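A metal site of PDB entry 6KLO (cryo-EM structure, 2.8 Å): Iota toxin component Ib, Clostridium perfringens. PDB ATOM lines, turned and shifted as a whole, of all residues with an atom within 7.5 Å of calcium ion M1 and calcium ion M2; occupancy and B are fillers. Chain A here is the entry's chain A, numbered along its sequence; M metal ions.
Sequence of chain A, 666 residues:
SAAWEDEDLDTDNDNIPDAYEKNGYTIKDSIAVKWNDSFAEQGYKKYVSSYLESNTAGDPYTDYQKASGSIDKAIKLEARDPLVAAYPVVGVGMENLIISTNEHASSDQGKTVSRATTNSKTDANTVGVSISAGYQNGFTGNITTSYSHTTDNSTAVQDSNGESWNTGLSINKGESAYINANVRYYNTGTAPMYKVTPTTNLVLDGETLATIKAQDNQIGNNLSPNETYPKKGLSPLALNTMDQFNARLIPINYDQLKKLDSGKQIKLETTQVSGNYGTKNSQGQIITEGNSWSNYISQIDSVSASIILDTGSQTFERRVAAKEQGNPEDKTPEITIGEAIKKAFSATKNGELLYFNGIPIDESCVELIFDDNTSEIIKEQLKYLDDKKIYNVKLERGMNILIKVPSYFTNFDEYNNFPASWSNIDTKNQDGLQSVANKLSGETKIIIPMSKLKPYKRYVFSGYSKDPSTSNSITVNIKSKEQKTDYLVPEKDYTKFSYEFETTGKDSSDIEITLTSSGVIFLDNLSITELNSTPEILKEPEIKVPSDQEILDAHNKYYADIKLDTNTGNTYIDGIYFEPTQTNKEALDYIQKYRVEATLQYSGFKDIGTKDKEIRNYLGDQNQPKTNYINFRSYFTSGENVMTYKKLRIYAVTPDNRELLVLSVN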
ATOM      1  N   LEU A   9       1.335   1.052 -11.434  1.00  0.00           N
ATOM      2  CA  LEU A   9      -0.008   1.165 -11.969  1.00  0.00           C
ATOM      3  C   LEU A   9       0.038   1.532 -13.450  1.00  0.00           C
ATOM      4  O   LEU A   9       0.878   2.316 -13.874  1.00  0.00           O
ATOM      5  CB  LEU A   9      -0.805   2.218 -11.195  1.00  0.00           C
ATOM      6  CG  LEU A   9      -2.204   2.576 -11.694  1.00  0.00           C
ATOM      7  CD1 LEU A   9      -3.128   1.377 -11.601  1.00  0.00           C
ATOM      8  CD2 LEU A   9      -2.751   3.742 -10.904  1.00  0.00           C
ATOM      9  N   ASP A  10      -0.883   0.952 -14.224  1.00  0.00           N
ATOM     10  CA  ASP A  10      -1.012   1.224 -15.659  1.00  0.00           C
ATOM     11  C   ASP A  10      -2.492   1.521 -15.916  1.00  0.00           C
ATOM     12  O   ASP A  10      -3.307   0.595 -15.965  1.00  0.00           O
ATOM     13  CB  ASP A  10      -0.518   0.042 -16.483  1.00  0.00           C
ATOM     14  CG  ASP A  10      -0.386   0.375 -17.946  1.00  0.00           C
ATOM     15  OD1 ASP A  10      -0.317   1.576 -18.286  1.00  0.00           O
ATOM     16  OD2 ASP A  10      -0.335  -0.572 -18.764  1.00  0.00           O
ATOM     17  N   THR A  11      -2.824   2.798 -16.077  1.00  0.00           N
ATOM     18  CA  THR A  11      -4.224   3.189 -16.159  1.00  0.00           C
ATOM     19  C   THR A  11      -4.800   2.896 -17.540  1.00  0.00           C
ATOM     20  O   THR A  11      -5.924   2.387 -17.664  1.00  0.00           O
ATOM     21  CB  THR A  11      -4.377   4.668 -15.816  1.00  0.00           C
ATOM     22  OG1 THR A  11      -3.929   4.894 -14.479  1.00  0.00           O
ATOM     23  CG2 THR A  11      -5.835   5.077 -15.920  1.00  0.00           C
ATOM     24  N   ASP A  12      -4.049   3.204 -18.599  1.00  0.00           N
ATOM     25  CA  ASP A  12      -4.547   3.016 -19.953  1.00  0.00           C
ATOM     26  C   ASP A  12      -4.241   1.638 -20.511  1.00  0.00           C
ATOM     27  O   ASP A  12      -4.636   1.357 -21.651  1.00  0.00           O
ATOM     28  CB  ASP A  12      -3.955   4.081 -20.878  1.00  0.00           C
ATOM     29  CG  ASP A  12      -2.481   4.274 -20.676  1.00  0.00           C
ATOM     30  OD1 ASP A  12      -1.932   3.664 -19.738  1.00  0.00           O
ATOM     31  OD2 ASP A  12      -1.869   5.030 -21.442  1.00  0.00           O
ATOM     32  N   ASN A  13      -3.564   0.774 -19.751  1.00  0.00           N
ATOM     33  CA  ASN A  13      -3.236  -0.593 -20.169  1.00  0.00           C
ATOM     34  C   ASN A  13      -2.530  -0.611 -21.517  1.00  0.00           C
ATOM     35  O   ASN A  13      -3.011  -1.160 -22.510  1.00  0.00           O
ATOM     36  CB  ASN A  13      -4.487  -1.469 -20.201  1.00  0.00           C
ATOM     37  CG  ASN A  13      -5.347  -1.326 -18.953  1.00  0.00           C
ATOM     38  OD1 ASN A  13      -4.925  -1.695 -17.862  1.00  0.00           O
ATOM     39  ND2 ASN A  13      -6.538  -0.786 -19.117  1.00  0.00           N
ATOM     40  N   ASP A  14      -1.351   0.025 -21.560  1.00  0.00           N
ATOM     41  CA  ASP A  14      -0.478  -0.050 -22.723  1.00  0.00           C
ATOM     42  C   ASP A  14       0.906  -0.574 -22.354  1.00  0.00           C
ATOM     43  O   ASP A  14       1.836  -0.442 -23.142  1.00  0.00           O
ATOM     44  CB  ASP A  14      -0.360   1.310 -23.415  1.00  0.00           C
ATOM     45  CG  ASP A  14       0.107   2.401 -22.479  1.00  0.00           C
ATOM     46  OD1 ASP A  14       0.172   2.167 -21.255  1.00  0.00           O
ATOM     47  OD2 ASP A  14       0.395   3.511 -22.967  1.00  0.00           O
ATOM     48  N   ASN A  15       1.044  -1.173 -21.169  1.00  0.00           N
ATOM     49  CA  ASN A  15       2.272  -1.800 -20.707  1.00  0.00           C
ATOM     50  C   ASN A  15       3.381  -0.791 -20.424  1.00  0.00           C
ATOM     51  O   ASN A  15       4.565  -1.116 -20.544  1.00  0.00           O
ATOM     52  CB  ASN A  15       2.766  -2.869 -21.688  1.00  0.00           C
ATOM     53  CG  ASN A  15       1.661  -3.799 -22.141  1.00  0.00           C
ATOM     54  OD1 ASN A  15       0.771  -4.147 -21.364  1.00  0.00           O
ATOM     55  ND2 ASN A  15       1.712  -4.208 -23.405  1.00  0.00           N
ATOM     56  N   ILE A  16       3.014   0.431 -20.058  1.00  0.00           N
ATOM     57  CA  ILE A  16       3.966   1.417 -19.565  1.00  0.00           C
ATOM     58  C   ILE A  16       3.337   2.060 -18.336  1.00  0.00           C
ATOM     59  O   ILE A  16       2.257   2.653 -18.434  1.00  0.00           O
ATOM     60  CB  ILE A  16       4.321   2.492 -20.609  1.00  0.00           C
ATOM     61  CG1 ILE A  16       4.601   1.862 -21.969  1.00  0.00           C
ATOM     62  CG2 ILE A  16       5.531   3.282 -20.157  1.00  0.00           C
ATOM     63  CD1 ILE A  16       4.722   2.867 -23.071  1.00  0.00           C
ATOM     64  N   PRO A  17       3.955   1.974 -17.166  1.00  0.00           N
ATOM     65  CA  PRO A  17       3.351   2.547 -15.957  1.00  0.00           C
ATOM     66  C   PRO A  17       3.152   4.045 -16.065  1.00  0.00           C
ATOM     67  O   PRO A  17       3.811   4.739 -16.854  1.00  0.00           O
ATOM     68  CB  PRO A  17       4.354   2.204 -14.851  1.00  0.00           C
ATOM     69  CG  PRO A  17       5.113   1.045 -15.390  1.00  0.00           C
ATOM     70  CD  PRO A  17       5.196   1.256 -16.860  1.00  0.00           C
ATOM     71  N   ASP A  18       2.225   4.564 -15.257  1.00  0.00           N
ATOM     72  CA  ASP A  18       1.912   5.986 -15.273  1.00  0.00           C
ATOM     73  C   ASP A  18       3.115   6.831 -14.899  1.00  0.00           C
ATOM     74  O   ASP A  18       3.390   7.863 -15.530  1.00  0.00           O
ATOM     75  CB  ASP A  18       0.754   6.289 -14.336  1.00  0.00           C
ATOM     76  CG  ASP A  18      -0.526   5.584 -14.738  1.00  0.00           C
ATOM     77  OD1 ASP A  18      -0.480   4.766 -15.673  1.00  0.00           O
ATOM     78  OD2 ASP A  18      -1.576   5.852 -14.117  1.00  0.00           O
ATOM     79  N   ALA A  19       3.839   6.437 -13.856  1.00  0.00           N
ATOM     80  CA  ALA A  19       5.002   7.205 -13.421  1.00  0.00           C
ATOM     81  C   ALA A  19       6.033   7.308 -14.520  1.00  0.00           C
ATOM     82  O   ALA A  19       6.613   8.383 -14.738  1.00  0.00           O
ATOM     83  CB  ALA A  19       5.612   6.569 -12.169  1.00  0.00           C
ATOM     84  N   GLU A  21       5.481   7.041 -17.835  1.00  0.00           N
ATOM     85  CA  GLU A  21       4.969   7.841 -18.946  1.00  0.00           C
ATOM     86  C   GLU A  21       4.935   9.326 -18.622  1.00  0.00           C
ATOM     87  O   GLU A  21       5.019  10.154 -19.525  1.00  0.00           O
ATOM     88  CB  GLU A  21       3.576   7.343 -19.343  1.00  0.00           C
ATOM     89  CG  GLU A  21       3.639   6.345 -20.478  1.00  0.00           C
ATOM     90  CD  GLU A  21       2.285   6.021 -21.044  1.00  0.00           C
ATOM     91  OE1 GLU A  21       1.284   6.217 -20.351  1.00  0.00           O
ATOM     92  OE2 GLU A  21       2.221   5.596 -22.216  1.00  0.00           O
ATOM     93  N   TYR A  25      10.888   7.468 -19.730  1.00  0.00           N
ATOM     94  CA  TYR A  25      11.191   6.045 -19.777  1.00  0.00           C
ATOM     95  C   TYR A  25      11.943   5.742 -21.063  1.00  0.00           C
ATOM     96  O   TYR A  25      12.024   6.573 -21.975  1.00  0.00           O
ATOM     97  CB  TYR A  25       9.928   5.204 -19.685  1.00  0.00           C
ATOM     98  CG  TYR A  25       8.986   5.371 -20.857  1.00  0.00           C
ATOM     99  CD1 TYR A  25       8.035   6.375 -20.868  1.00  0.00           C
ATOM    100  CD2 TYR A  25       9.042   4.523 -21.948  1.00  0.00           C
ATOM    101  CE1 TYR A  25       7.174   6.536 -21.923  1.00  0.00           C
ATOM    102  CE2 TYR A  25       8.188   4.677 -23.008  1.00  0.00           C
ATOM    103  CZ  TYR A  25       7.252   5.678 -22.991  1.00  0.00           C
ATOM    104  OH  TYR A  25       6.392   5.839 -24.046  1.00  0.00           O
ATOM    105  N   SER A  49       4.824  10.376 -22.492  1.00  0.00           N
ATOM    106  CA  SER A  49       3.544  10.077 -23.102  1.00  0.00           C
ATOM    107  C   SER A  49       2.428  10.451 -22.140  1.00  0.00           C
ATOM    108  O   SER A  49       2.655  10.747 -20.970  1.00  0.00           O
ATOM    109  CB  SER A  49       3.432   8.604 -23.480  1.00  0.00           C
ATOM    110  OG  SER A  49       4.410   8.246 -24.442  1.00  0.00           O
ATOM    111  N   SER A  50       1.209  10.431 -22.657  1.00  0.00           N
ATOM    112  CA  SER A  50       0.029  10.589 -21.819  1.00  0.00           C
ATOM    113  C   SER A  50      -0.251   9.282 -21.098  1.00  0.00           C
ATOM    114  O   SER A  50      -0.351   8.219 -21.719  1.00  0.00           O
ATOM    115  CB  SER A  50      -1.170  10.992 -22.664  1.00  0.00           C
ATOM    116  OG  SER A  50      -2.259  11.390 -21.844  1.00  0.00           O
ATOM    117  N   TYR A  51      -0.381   9.349 -19.780  1.00  0.00           N
ATOM    118  CA  TYR A  51      -0.689   8.141 -19.015  1.00  0.00           C
ATOM    119  C   TYR A  51      -2.171   7.826 -19.006  1.00  0.00           C
ATOM    120  O   TYR A  51      -2.579   6.861 -18.348  1.00  0.00           O
ATOM    121  CB  TYR A  51      -0.148   8.263 -17.587  1.00  0.00           C
ATOM    122  CG  TYR A  51      -0.884   9.245 -16.702  1.00  0.00           C
ATOM    123  CD1 TYR A  51      -0.523  10.579 -16.670  1.00  0.00           C
ATOM    124  CD2 TYR A  51      -1.924   8.820 -15.889  1.00  0.00           C
ATOM    125  CE1 TYR A  51      -1.188  11.462 -15.860  1.00  0.00           C
ATOM    126  CE2 TYR A  51      -2.589   9.703 -15.079  1.00  0.00           C
ATOM    127  CZ  TYR A  51      -2.209  11.018 -15.059  1.00  0.00           C
ATOM    128  OH  TYR A  51      -2.884  11.910 -14.254  1.00  0.00           O
ATOM    129  N   LEU A  52      -2.985   8.600 -19.716  1.00  0.00           N
ATOM    130  CA  LEU A  52      -4.413   8.339 -19.856  1.00  0.00           C
ATOM    131  C   LEU A  52      -4.806   8.017 -21.296  1.00  0.00           C
ATOM    132  O   LEU A  52      -5.999   7.912 -21.588  1.00  0.00           O
ATOM    133  CB  LEU A  52      -5.220   9.537 -19.357  1.00  0.00           C
ATOM    134  CG  LEU A  52      -5.234   9.805 -17.857  1.00  0.00           C
ATOM    135  CD1 LEU A  52      -6.136  10.985 -17.556  1.00  0.00           C
ATOM    136  CD2 LEU A  52      -5.680   8.583 -17.093  1.00  0.00           C
ATOM    137  N   GLU A  53      -3.836   7.866 -22.183  1.00  0.00           N
ATOM    138  CA  GLU A  53      -4.087   7.551 -23.583  1.00  0.00           C
ATOM    139  C   GLU A  53      -3.147   6.458 -24.038  1.00  0.00           C
ATOM    140  O   GLU A  53      -1.934   6.529 -23.786  1.00  0.00           O
ATOM    141  CB  GLU A  53      -3.910   8.775 -24.481  1.00  0.00           C
ATOM    142  CG  GLU A  53      -5.091   9.729 -24.480  1.00  0.00           C
ATOM    143  CD  GLU A  53      -6.204   9.260 -25.392  1.00  0.00           C
ATOM    144  OE1 GLU A  53      -5.946   8.389 -26.251  1.00  0.00           O
ATOM    145  OE2 GLU A  53      -7.341   9.766 -25.243  1.00  0.00           O
ATOM    146  N   SER A  54      -3.685   5.439 -24.710  1.00  0.00           N
ATOM    147  CA  SER A  54      -2.841   4.412 -25.302  1.00  0.00           C
ATOM    148  C   SER A  54      -2.201   4.896 -26.598  1.00  0.00           C
ATOM    149  O   SER A  54      -1.139   4.397 -26.976  1.00  0.00           O
ATOM    150  CB  SER A  54      -3.646   3.154 -25.569  1.00  0.00           C
ATOM    151  OG  SER A  54      -4.097   2.578 -24.368  1.00  0.00           O
ATOM    152  N   ASN A  55      -2.835   5.842 -27.274  1.00  0.00           N
ATOM    153  CA  ASN A  55      -2.373   6.381 -28.546  1.00  0.00           C
ATOM    154  C   ASN A  55      -2.269   7.889 -28.361  1.00  0.00           C
ATOM    155  O   ASN A  55      -3.214   8.628 -28.653  1.00  0.00           O
ATOM    156  CB  ASN A  55      -3.308   6.016 -29.689  1.00  0.00           C
ATOM    157  CG  ASN A  55      -3.317   4.530 -29.980  1.00  0.00           C
ATOM    158  OD1 ASN A  55      -2.589   4.065 -30.846  1.00  0.00           O
ATOM    159  ND2 ASN A  55      -4.160   3.803 -29.283  1.00  0.00           N
ATOM    160  N   THR A  56      -1.124   8.337 -27.859  1.00  0.00           N
ATOM    161  CA  THR A  56      -0.956   9.757 -27.580  1.00  0.00           C
ATOM    162  C   THR A  56      -0.998  10.596 -28.850  1.00  0.00           C
ATOM    163  O   THR A  56      -1.652  11.638 -28.895  1.00  0.00           O
ATOM    164  CB  THR A  56       0.349   9.991 -26.825  1.00  0.00           C
ATOM    165  OG1 THR A  56       0.274   9.376 -25.532  1.00  0.00           O
ATOM    166  CG2 THR A  56       0.619  11.470 -26.652  1.00  0.00           C
ATOM    167  N   THR A  62       0.228   2.127 -30.622  1.00  0.00           N
ATOM    168  CA  THR A  62       0.222   2.568 -29.239  1.00  0.00           C
ATOM    169  C   THR A  62       1.571   3.141 -28.836  1.00  0.00           C
ATOM    170  O   THR A  62       2.555   3.068 -29.580  1.00  0.00           O
ATOM    171  CB  THR A  62      -0.159   1.425 -28.300  1.00  0.00           C
ATOM    172  OG1 THR A  62       0.954   0.547 -28.136  1.00  0.00           O
ATOM    173  CG2 THR A  62      -1.322   0.636 -28.852  1.00  0.00           C
ATOM    174  N   ASP A  63       1.605   3.742 -27.649  1.00  0.00           N
ATOM    175  CA  ASP A  63       2.853   4.313 -27.132  1.00  0.00           C
ATOM    176  C   ASP A  63       3.936   3.250 -27.013  1.00  0.00           C
ATOM    177  O   ASP A  63       5.098   3.487 -27.356  1.00  0.00           O
ATOM    178  CB  ASP A  63       2.611   4.977 -25.792  1.00  0.00           C
ATOM    179  CG  ASP A  63       1.577   6.072 -25.858  1.00  0.00           C
ATOM    180  OD1 ASP A  63       1.265   6.531 -26.968  1.00  0.00           O
ATOM    181  OD2 ASP A  63       1.064   6.487 -24.794  1.00  0.00           O
ATOM    182  N   TYR A  64       3.561   2.058 -26.531  1.00  0.00           N
ATOM    183  CA  TYR A  64       4.550   1.003 -26.352  1.00  0.00           C
ATOM    184  C   TYR A  64       4.995   0.431 -27.692  1.00  0.00           C
ATOM    185  O   TYR A  64       6.181   0.153 -27.884  1.00  0.00           O
ATOM    186  CB  TYR A  64       4.002  -0.104 -25.464  1.00  0.00           C
ATOM    187  CG  TYR A  64       4.939  -1.275 -25.355  1.00  0.00           C
ATOM    188  CD1 TYR A  64       6.063  -1.203 -24.552  1.00  0.00           C
ATOM    189  CD2 TYR A  64       4.728  -2.432 -26.077  1.00  0.00           C
ATOM    190  CE1 TYR A  64       6.934  -2.258 -24.461  1.00  0.00           C
ATOM    191  CE2 TYR A  64       5.589  -3.491 -25.995  1.00  0.00           C
ATOM    192  CZ  TYR A  64       6.694  -3.399 -25.180  1.00  0.00           C
ATOM    193  OH  TYR A  64       7.568  -4.458 -25.080  1.00  0.00           O
ATOM    194  N   PRO A  82       6.618   8.605 -29.155  1.00  0.00           N
ATOM    195  CA  PRO A  82       5.162   8.642 -28.930  1.00  0.00           C
ATOM    196  C   PRO A  82       4.516   9.994 -29.165  1.00  0.00           C
ATOM    197  O   PRO A  82       3.289  10.066 -29.177  1.00  0.00           O
ATOM    198  CB  PRO A  82       5.025   8.213 -27.468  1.00  0.00           C
ATOM    199  CG  PRO A  82       6.245   7.432 -27.189  1.00  0.00           C
ATOM    200  CD  PRO A  82       7.334   8.051 -27.991  1.00  0.00           C
HETATM  201 CA    CA M   1      -0.053   6.011 -22.588  1.00  0.00          CA
HETATM  202 CA    CA M   2       0.370   3.646 -19.442  1.00  0.00          CA
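The side-chain hydroxyl (OG1) of Thr 56 is in hydrogen-bond range of the backbone NH (N) of Ser 50, 3.2 Å away. N of Thr 56 is in hydrogen-bond range of OD1 of Asp 63, 3.1 Å away. N of Asn 15 lies within hydrogen-bond range of OD2 of Asp 10, 2.8 Å away. The side-chain hydroxyl (OG) of Ser 54 lies within hydrogen-bond range of the backbone carbonyl oxygen (O) of Asp 12, 3.0 Å away. The backbone NH of Asp 63 lies within hydrogen-bond range of the backbone carbonyl oxygen of Ser 54 (2.9 Å). N of Ser 49 is in hydrogen-bond range of O of Glu 21 (3.0 Å). O of Asp 10 sits close to OD1 of Asn 13, at 3.4 Å.
O of Glu 53 binds calcium ion M1, 2.3 Å away. OE2 of Glu 21 binds calcium ion M1 (2.3 Å). Calcium ion M1 is bound by the side-chain carboxylate (OD2) of Asp 12, at 2.4 Å. Calcium ion M1 is bound by O of Ser 50. OD2 of Asp 63 is bound to calcium ion M1 (2.5 Å). Calcium ion M1 is bound by the side-chain carboxylate (OD2) of Asp 14 (2.6 Å). OE1 of Glu 21 binds calcium ion M1. Calcium ion M1 has seven donor atoms within binding distance.
Calcium ion M2 is bound by OD1 of Asp 12 (2.3 Å), OD1 of Asp 14 (2.3 Å), O of Ile 16 (2.4 Å), OD1 of Asp 10 (2.5 Å) and OE1 of Glu 21 (2.9 Å). Calcium ion M2 has five donor atoms within binding distance.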
